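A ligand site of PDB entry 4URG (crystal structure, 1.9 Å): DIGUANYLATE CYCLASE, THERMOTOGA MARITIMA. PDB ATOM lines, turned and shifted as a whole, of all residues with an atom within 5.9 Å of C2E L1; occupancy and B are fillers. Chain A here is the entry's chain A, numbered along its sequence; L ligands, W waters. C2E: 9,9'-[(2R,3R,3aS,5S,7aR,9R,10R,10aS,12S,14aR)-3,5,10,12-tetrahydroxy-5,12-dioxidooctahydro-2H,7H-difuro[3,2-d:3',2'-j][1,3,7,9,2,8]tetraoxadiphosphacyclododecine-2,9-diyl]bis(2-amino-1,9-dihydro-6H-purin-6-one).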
ATOM      1  N   ARG A  67     -24.717  25.421   9.118  1.00  0.00           N
ATOM      2  CA  ARG A  67     -24.767  26.390  10.217  1.00  0.00           C
ATOM      3  C   ARG A  67     -25.068  25.814  11.583  1.00  0.00           C
ATOM      4  O   ARG A  67     -25.192  26.558  12.549  1.00  0.00           O
ATOM      5  CB  ARG A  67     -25.706  27.562   9.875  1.00  0.00           C
ATOM      6  CG  ARG A  67     -25.165  28.474   8.763  1.00  0.00           C
ATOM      7  CD  ARG A  67     -24.234  29.568   9.273  1.00  0.00           C
ATOM      8  NE  ARG A  67     -22.960  29.528   8.563  1.00  0.00           N
ATOM      9  CZ  ARG A  67     -22.704  30.162   7.420  1.00  0.00           C
ATOM     10  NH1 ARG A  67     -23.638  30.918   6.850  1.00  0.00           N
ATOM     11  NH2 ARG A  67     -21.524  30.041   6.837  1.00  0.00           N
ATOM     12  N   VAL A  68     -25.173  24.483  11.663  1.00  0.00           N
ATOM     13  CA  VAL A  68     -25.345  23.771  12.933  1.00  0.00           C
ATOM     14  C   VAL A  68     -24.245  22.738  13.020  1.00  0.00           C
ATOM     15  O   VAL A  68     -23.671  22.371  11.998  1.00  0.00           O
ATOM     16  CB  VAL A  68     -26.756  23.162  13.177  1.00  0.00           C
ATOM     17  CG1 VAL A  68     -27.857  24.216  13.029  1.00  0.00           C
ATOM     18  CG2 VAL A  68     -27.024  21.968  12.266  1.00  0.00           C
ATOM     19  N   ARG A  69     -23.951  22.241  14.228  1.00  0.00           N
ATOM     20  CA  ARG A  69     -22.903  21.221  14.372  1.00  0.00           C
ATOM     21  C   ARG A  69     -23.236  19.918  13.680  1.00  0.00           C
ATOM     22  O   ARG A  69     -24.397  19.524  13.631  1.00  0.00           O
ATOM     23  CB  ARG A  69     -22.618  20.953  15.870  1.00  0.00           C
ATOM     24  CG  ARG A  69     -22.165  22.225  16.566  1.00  0.00           C
ATOM     25  CD  ARG A  69     -21.600  22.021  17.934  1.00  0.00           C
ATOM     26  NE  ARG A  69     -21.194  23.335  18.463  1.00  0.00           N
ATOM     27  CZ  ARG A  69     -20.760  23.529  19.689  1.00  0.00           C
ATOM     28  NH1 ARG A  69     -20.679  22.529  20.550  1.00  0.00           N
ATOM     29  NH2 ARG A  69     -20.429  24.754  20.090  1.00  0.00           N
ATOM     30  N   ASP A  72     -25.153  17.791  15.777  1.00  0.00           N
ATOM     31  CA  ASP A  72     -26.586  18.109  15.942  1.00  0.00           C
ATOM     32  C   ASP A  72     -27.344  17.358  14.849  1.00  0.00           C
ATOM     33  O   ASP A  72     -26.738  16.887  13.876  1.00  0.00           O
ATOM     34  CB  ASP A  72     -26.858  19.624  15.842  1.00  0.00           C
ATOM     35  CG  ASP A  72     -26.197  20.450  16.923  1.00  0.00           C
ATOM     36  OD1 ASP A  72     -26.124  19.975  18.070  1.00  0.00           O
ATOM     37  OD2 ASP A  72     -25.742  21.563  16.614  1.00  0.00           O
ATOM     38  N   LEU A  86     -30.577  20.090  19.120  1.00  0.00           N
ATOM     39  CA  LEU A  86     -29.331  20.719  19.522  1.00  0.00           C
ATOM     40  C   LEU A  86     -28.941  20.128  20.861  1.00  0.00           C
ATOM     41  O   LEU A  86     -29.590  20.387  21.875  1.00  0.00           O
ATOM     42  CB  LEU A  86     -29.488  22.243  19.655  1.00  0.00           C
ATOM     43  CG  LEU A  86     -29.992  23.035  18.453  1.00  0.00           C
ATOM     44  CD1 LEU A  86     -30.411  24.463  18.909  1.00  0.00           C
ATOM     45  CD2 LEU A  86     -28.938  23.077  17.345  1.00  0.00           C
ATOM     46  N   TYR A  87     -27.876  19.315  20.842  1.00  0.00           N
ATOM     47  CA  TYR A  87     -27.342  18.632  22.008  1.00  0.00           C
ATOM     48  C   TYR A  87     -26.524  19.577  22.871  1.00  0.00           C
ATOM     49  O   TYR A  87     -25.697  20.346  22.389  1.00  0.00           O
ATOM     50  CB  TYR A  87     -26.533  17.382  21.582  1.00  0.00           C
ATOM     51  CG  TYR A  87     -26.117  16.547  22.756  1.00  0.00           C
ATOM     52  CD1 TYR A  87     -26.956  15.566  23.282  1.00  0.00           C
ATOM     53  CD2 TYR A  87     -24.880  16.756  23.395  1.00  0.00           C
ATOM     54  CE1 TYR A  87     -26.600  14.823  24.396  1.00  0.00           C
ATOM     55  CE2 TYR A  87     -24.517  16.035  24.518  1.00  0.00           C
ATOM     56  CZ  TYR A  87     -25.369  15.042  24.996  1.00  0.00           C
ATOM     57  OH  TYR A  87     -25.038  14.317  26.108  1.00  0.00           O
ATOM     58  N   ASP A  88     -26.752  19.515  24.176  1.00  0.00           N
ATOM     59  CA  ASP A  88     -26.024  20.261  25.162  1.00  0.00           C
ATOM     60  C   ASP A  88     -26.138  21.759  24.959  1.00  0.00           C
ATOM     61  O   ASP A  88     -25.170  22.503  24.794  1.00  0.00           O
ATOM     62  CB  ASP A  88     -24.593  19.719  25.322  1.00  0.00           C
ATOM     63  CG  ASP A  88     -23.766  20.378  26.410  1.00  0.00           C
ATOM     64  OD1 ASP A  88     -24.350  20.934  27.373  1.00  0.00           O
ATOM     65  OD2 ASP A  88     -22.552  20.385  26.283  1.00  0.00           O
ATOM     66  N   MET A  89     -27.386  22.194  25.043  1.00  0.00           N
ATOM     67  CA  MET A  89     -27.741  23.582  24.887  1.00  0.00           C
ATOM     68  C   MET A  89     -28.122  24.180  26.217  1.00  0.00           C
ATOM     69  O   MET A  89     -28.403  23.450  27.159  1.00  0.00           O
ATOM     70  CB  MET A  89     -28.858  23.754  23.840  1.00  0.00           C
ATOM     71  CG  MET A  89     -28.361  24.221  22.499  1.00  0.00           C
ATOM     72  SD  MET A  89     -27.641  25.883  22.455  1.00  0.00           S
ATOM     73  CE  MET A  89     -29.088  26.863  22.453  1.00  0.00           C
ATOM     74  N   LYS A  90     -28.115  25.505  26.305  1.00  0.00           N
ATOM     75  CA  LYS A  90     -28.516  26.209  27.506  1.00  0.00           C
ATOM     76  C   LYS A  90     -29.356  27.365  27.057  1.00  0.00           C
ATOM     77  O   LYS A  90     -29.186  27.879  25.939  1.00  0.00           O
ATOM     78  CB  LYS A  90     -27.290  26.737  28.299  1.00  0.00           C
ATOM     79  CG  LYS A  90     -26.445  25.684  29.025  1.00  0.00           C
ATOM     80  CD  LYS A  90     -25.334  26.361  29.828  1.00  0.00           C
ATOM     81  CE  LYS A  90     -23.928  25.907  29.463  1.00  0.00           C
ATOM     82  NZ  LYS A  90     -22.899  27.006  29.587  1.00  0.00           N
ATOM     83  N   TYR A  93     -27.934  30.687  25.530  1.00  0.00           N
ATOM     84  CA  TYR A  93     -27.415  30.731  24.152  1.00  0.00           C
ATOM     85  C   TYR A  93     -28.502  30.601  23.092  1.00  0.00           C
ATOM     86  O   TYR A  93     -28.215  30.721  21.902  1.00  0.00           O
ATOM     87  CB  TYR A  93     -26.362  29.640  23.963  1.00  0.00           C
ATOM     88  CG  TYR A  93     -25.336  29.590  25.089  1.00  0.00           C
ATOM     89  CD1 TYR A  93     -24.618  30.739  25.443  1.00  0.00           C
ATOM     90  CD2 TYR A  93     -25.036  28.400  25.737  1.00  0.00           C
ATOM     91  CE1 TYR A  93     -23.681  30.696  26.486  1.00  0.00           C
ATOM     92  CE2 TYR A  93     -24.079  28.349  26.741  1.00  0.00           C
ATOM     93  CZ  TYR A  93     -23.421  29.498  27.128  1.00  0.00           C
ATOM     94  OH  TYR A  93     -22.476  29.444  28.114  1.00  0.00           O
ATOM     95  N   SER A  96     -29.265  33.525  20.385  1.00  0.00           N
ATOM     96  CA  SER A  96     -28.247  33.525  19.327  1.00  0.00           C
ATOM     97  C   SER A  96     -28.469  32.416  18.303  1.00  0.00           C
ATOM     98  O   SER A  96     -28.365  32.660  17.101  1.00  0.00           O
ATOM     99  CB  SER A  96     -26.817  33.476  19.909  1.00  0.00           C
ATOM    100  OG  SER A  96     -26.428  32.177  20.350  1.00  0.00           O
ATOM    101  N   LEU A  97     -28.853  31.209  18.764  1.00  0.00           N
ATOM    102  CA  LEU A  97     -29.141  30.071  17.876  1.00  0.00           C
ATOM    103  C   LEU A  97     -30.349  30.313  16.999  1.00  0.00           C
ATOM    104  O   LEU A  97     -30.318  29.986  15.806  1.00  0.00           O
ATOM    105  CB  LEU A  97     -29.313  28.740  18.665  1.00  0.00           C
ATOM    106  CG  LEU A  97     -28.078  27.838  18.848  1.00  0.00           C
ATOM    107  CD1 LEU A  97     -27.606  27.221  17.512  1.00  0.00           C
ATOM    108  CD2 LEU A  97     -26.934  28.552  19.595  1.00  0.00           C
ATOM    109  N   ARG A 100     -29.450  32.881  14.242  1.00  0.00           N
ATOM    110  CA  ARG A 100     -28.651  32.230  13.204  1.00  0.00           C
ATOM    111  C   ARG A 100     -29.525  31.353  12.284  1.00  0.00           C
ATOM    112  O   ARG A 100     -29.368  31.408  11.066  1.00  0.00           O
ATOM    113  CB  ARG A 100     -27.563  31.358  13.852  1.00  0.00           C
ATOM    114  CG  ARG A 100     -26.530  30.805  12.884  1.00  0.00           C
ATOM    115  CD  ARG A 100     -25.835  29.557  13.435  1.00  0.00           C
ATOM    116  NE  ARG A 100     -25.294  29.756  14.780  1.00  0.00           N
ATOM    117  CZ  ARG A 100     -24.920  28.789  15.598  1.00  0.00           C
ATOM    118  NH1 ARG A 100     -24.979  27.515  15.208  1.00  0.00           N
ATOM    119  NH2 ARG A 100     -24.463  29.067  16.815  1.00  0.00           N
HETATM  120  P1  C2E L   1     -18.978  26.693  23.224  1.00  0.00           P
HETATM  121  O2P C2E L   1     -18.117  26.726  24.463  1.00  0.00           O
HETATM  122  O1P C2E L   1     -19.058  25.392  22.543  1.00  0.00           O
HETATM  123  O5' C2E L   1     -18.450  27.815  22.222  1.00  0.00           O
HETATM  124  C5' C2E L   1     -18.071  29.120  22.706  1.00  0.00           C
HETATM  125  C4' C2E L   1     -17.853  30.099  21.565  1.00  0.00           C
HETATM  126  O4' C2E L   1     -16.858  29.616  20.665  1.00  0.00           O
HETATM  127  C3' C2E L   1     -19.097  30.240  20.723  1.00  0.00           C
HETATM  128  O3' C2E L   1     -20.040  31.141  21.348  1.00  0.00           O
HETATM  129  C2' C2E L   1     -18.542  30.769  19.422  1.00  0.00           C
HETATM  130  O2' C2E L   1     -18.152  32.182  19.525  1.00  0.00           O
HETATM  131  C1' C2E L   1     -17.293  29.926  19.324  1.00  0.00           C
HETATM  132  N9  C2E L   1     -17.493  28.652  18.535  1.00  0.00           N
HETATM  133  C8  C2E L   1     -17.418  27.408  19.011  1.00  0.00           C
HETATM  134  N7  C2E L   1     -17.515  26.550  17.980  1.00  0.00           N
HETATM  135  C5  C2E L   1     -17.662  27.299  16.877  1.00  0.00           C
HETATM  136  C6  C2E L   1     -17.876  26.990  15.586  1.00  0.00           C
HETATM  137  O6  C2E L   1     -17.849  25.682  15.248  1.00  0.00           O
HETATM  138  N1  C2E L   1     -17.908  27.941  14.653  1.00  0.00           N
HETATM  139  C2  C2E L   1     -17.913  29.251  14.983  1.00  0.00           C
HETATM  140  N2  C2E L   1     -17.967  30.173  14.013  1.00  0.00           N
HETATM  141  N3  C2E L   1     -17.732  29.585  16.270  1.00  0.00           N
HETATM  142  C4  C2E L   1     -17.564  28.603  17.213  1.00  0.00           C
HETATM  143  P11 C2E L   1     -21.575  31.193  20.932  1.00  0.00           P
HETATM  144  O21 C2E L   1     -21.754  31.116  19.469  1.00  0.00           O
HETATM  145  O11 C2E L   1     -22.122  32.370  21.627  1.00  0.00           O
HETATM  146  O5A C2E L   1     -22.255  29.881  21.564  1.00  0.00           O
HETATM  147  C5A C2E L   1     -22.204  29.650  22.997  1.00  0.00           C
HETATM  148  C4A C2E L   1     -22.552  28.217  23.326  1.00  0.00           C
HETATM  149  O4A C2E L   1     -23.778  27.850  22.620  1.00  0.00           O
HETATM  150  C3A C2E L   1     -21.545  27.260  22.820  1.00  0.00           C
HETATM  151  O3A C2E L   1     -20.393  27.200  23.742  1.00  0.00           O
HETATM  152  C2A C2E L   1     -22.311  25.990  22.818  1.00  0.00           C
HETATM  153  O2A C2E L   1     -22.423  25.437  24.180  1.00  0.00           O
HETATM  154  C1A C2E L   1     -23.685  26.456  22.298  1.00  0.00           C
HETATM  155  N91 C2E L   1     -23.781  26.386  20.803  1.00  0.00           N
HETATM  156  C81 C2E L   1     -23.612  27.374  19.915  1.00  0.00           C
HETATM  157  N71 C2E L   1     -23.881  26.926  18.675  1.00  0.00           N
HETATM  158  C51 C2E L   1     -24.214  25.631  18.798  1.00  0.00           C
HETATM  159  C61 C2E L   1     -24.628  24.699  17.914  1.00  0.00           C
HETATM  160  O61 C2E L   1     -24.624  25.000  16.603  1.00  0.00           O
HETATM  161  N11 C2E L   1     -24.971  23.468  18.316  1.00  0.00           N
HETATM  162  C21 C2E L   1     -24.919  23.148  19.631  1.00  0.00           C
HETATM  163  N21 C2E L   1     -25.296  21.949  20.013  1.00  0.00           N
HETATM  164  N31 C2E L   1     -24.528  24.084  20.544  1.00  0.00           N
HETATM  165  C41 C2E L   1     -24.190  25.317  20.119  1.00  0.00           C
HETATM  166  P1  C2E L   2     -17.588  26.931  10.921  1.00  0.00           P
HETATM  167  O2P C2E L   2     -17.109  27.255   9.561  1.00  0.00           O
HETATM  168  O1P C2E L   2     -17.486  27.971  11.965  1.00  0.00           O
HETATM  169  O5' C2E L   2     -16.759  25.662  11.429  1.00  0.00           O
HETATM  170  C5' C2E L   2     -16.519  24.533  10.554  1.00  0.00           C
HETATM  171  C4' C2E L   2     -15.993  23.384  11.368  1.00  0.00           C
HETATM  172  O4' C2E L   2     -14.761  23.778  12.009  1.00  0.00           O
HETATM  173  C3' C2E L   2     -16.948  23.064  12.522  1.00  0.00           C
HETATM  174  O3' C2E L   2     -17.980  22.179  12.055  1.00  0.00           O
HETATM  175  C2' C2E L   2     -16.021  22.399  13.499  1.00  0.00           C
HETATM  176  O2' C2E L   2     -15.718  21.001  13.062  1.00  0.00           O
HETATM  177  C1' C2E L   2     -14.755  23.290  13.342  1.00  0.00           C
HETATM  178  N9  C2E L   2     -14.715  24.401  14.304  1.00  0.00           N
HETATM  179  C8  C2E L   2     -14.786  25.720  14.060  1.00  0.00           C
HETATM  180  N7  C2E L   2     -14.652  26.350  15.213  1.00  0.00           N
HETATM  181  C5  C2E L   2     -14.538  25.438  16.181  1.00  0.00           C
HETATM  182  C6  C2E L   2     -14.311  25.507  17.488  1.00  0.00           C
HETATM  183  O6  C2E L   2     -14.208  26.733  18.036  1.00  0.00           O
HETATM  184  N1  C2E L   2     -14.197  24.410  18.251  1.00  0.00           N
HETATM  185  C2  C2E L   2     -14.206  23.194  17.690  1.00  0.00           C
HETATM  186  N2  C2E L   2     -14.079  22.112  18.464  1.00  0.00           N
HETATM  187  N3  C2E L   2     -14.374  23.101  16.365  1.00  0.00           N
HETATM  188  C4  C2E L   2     -14.502  24.230  15.612  1.00  0.00           C
HETATM  189  P11 C2E L   2     -19.328  21.941  12.940  1.00  0.00           P
HETATM  190  O21 C2E L   2     -19.008  21.688  14.346  1.00  0.00           O
HETATM  191  O11 C2E L   2     -20.070  20.854  12.196  1.00  0.00           O
HETATM  192  O5A C2E L   2     -20.119  23.262  12.847  1.00  0.00           O
HETATM  193  C5A C2E L   2     -20.632  23.701  11.530  1.00  0.00           C
HETATM  194  C4A C2E L   2     -21.046  25.181  11.569  1.00  0.00           C
HETATM  195  O4A C2E L   2     -22.017  25.390  12.610  1.00  0.00           O
HETATM  196  C3A C2E L   2     -19.891  26.104  11.912  1.00  0.00           C
HETATM  197  O3A C2E L   2     -19.078  26.373  10.763  1.00  0.00           O
HETATM  198  C2A C2E L   2     -20.653  27.353  12.383  1.00  0.00           C
HETATM  199  O2A C2E L   2     -21.219  28.099  11.288  1.00  0.00           O
HETATM  200  C1A C2E L   2     -21.814  26.701  13.160  1.00  0.00           C
HETATM  201  N91 C2E L   2     -21.472  26.530  14.594  1.00  0.00           N
HETATM  202  C81 C2E L   2     -21.180  25.384  15.231  1.00  0.00           C
HETATM  203  N71 C2E L   2     -20.994  25.658  16.528  1.00  0.00           N
HETATM  204  C51 C2E L   2     -21.147  26.974  16.674  1.00  0.00           C
HETATM  205  C61 C2E L   2     -20.929  27.811  17.701  1.00  0.00           C
HETATM  206  O61 C2E L   2     -20.667  27.291  18.921  1.00  0.00           O
HETATM  207  N11 C2E L   2     -21.111  29.125  17.569  1.00  0.00           N
HETATM  208  C21 C2E L   2     -21.383  29.663  16.390  1.00  0.00           C
HETATM  209  N21 C2E L   2     -21.552  30.960  16.300  1.00  0.00           N
HETATM  210  N31 C2E L   2     -21.544  28.850  15.329  1.00  0.00           N
HETATM  211  C41 C2E L   2     -21.373  27.515  15.466  1.00  0.00           C
HETATM  212  O   HOH W   1     -20.321  22.812  23.376  1.00  0.00           O
HETATM  213  O   HOH W   2     -16.563  32.884  17.600  1.00  0.00           O
HETATM  214  O   HOH W   3     -24.373  31.467  18.462  1.00  0.00           O
HETATM  215  O   HOH W   4     -23.293  22.539  22.756  1.00  0.00           O
HETATM  216  O   HOH W   5     -20.994  25.689  26.309  1.00  0.00           O
HETATM  217  O   HOH W   6     -17.701  32.687  15.367  1.00  0.00           O
HETATM  218  O   HOH W   7     -17.003  23.894  21.552  1.00  0.00           O
HETATM  219  O   HOH W   8     -24.420  24.911  25.918  1.00  0.00           O
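The side-chain carboxylate of Asp 72 sits at hydrogen-bond distance from the backbone NH of Arg 69 (3.1 Å).
OD1 of Asp 72 sits at hydrogen-bond distance from N of Tyr 87.
O of Arg 67 is in hydrogen-bond range of NH1 of Arg 100, at 2.8 Å.
The backbone carbonyl oxygen of Tyr 93 lies within hydrogen-bond range of the side-chain hydroxyl of Ser 96 (2.8 Å).
The side-chain hydroxyl (OH) of Tyr 93 sits at hydrogen-bond distance from the side-chain amino group (NZ) of Lys 90 (2.9 Å).
Residues that only touch C2E L1: Tyr 93 (3.4 Å), Leu 97 (3.5 Å) and Val 68 (3.9 Å).
A nitrogen (N1) of C2E L1 lies within hydrogen-bond range of an oxygen (O1P) of C2E L2 (2.7 Å).
OD2 of Asp 72 lies within hydrogen-bond range of N11 of C2E L1 (2.7 Å).
NH2 of Arg 69 lies within salt-bridge range of O1P of C2E L1 (2.9 Å).
The backbone carbonyl oxygen (O) of Tyr 87 lies within hydrogen-bond range of a nitrogen (N21) of C2E L1 (2.9 Å).
The guanidinium group of Arg 100 sits at hydrogen-bond distance from a nitrogen (N71) of C2E L1.
O61 of C2E L2 is in hydrogen-bond range of NH2 of Arg 69 (2.8 Å).
The guanidinium group (NH2) of Arg 100 sits close to a nitrogen (N31) of C2E L2 (3.3 Å).
An oxygen (O4A) of C2E L2 sits at hydrogen-bond distance from the backbone NH (N) of Val 68, 3.4 Å away.
Water W8 lies within hydrogen-bond range of O2A of C2E L1 (2.7 Å) and O of Asp 88 (2.8 Å).
Water W3 lies within hydrogen-bond range of an oxygen (O21) of C2E L1, the side-chain hydroxyl (OG) of Ser 96 and the guanidinium group (NH2) of Arg 100.
Water W1 lies within hydrogen-bond range of the guanidinium group of Arg 69 (2.9 Å) and an oxygen (O1P) of C2E L1 (3.0 Å).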
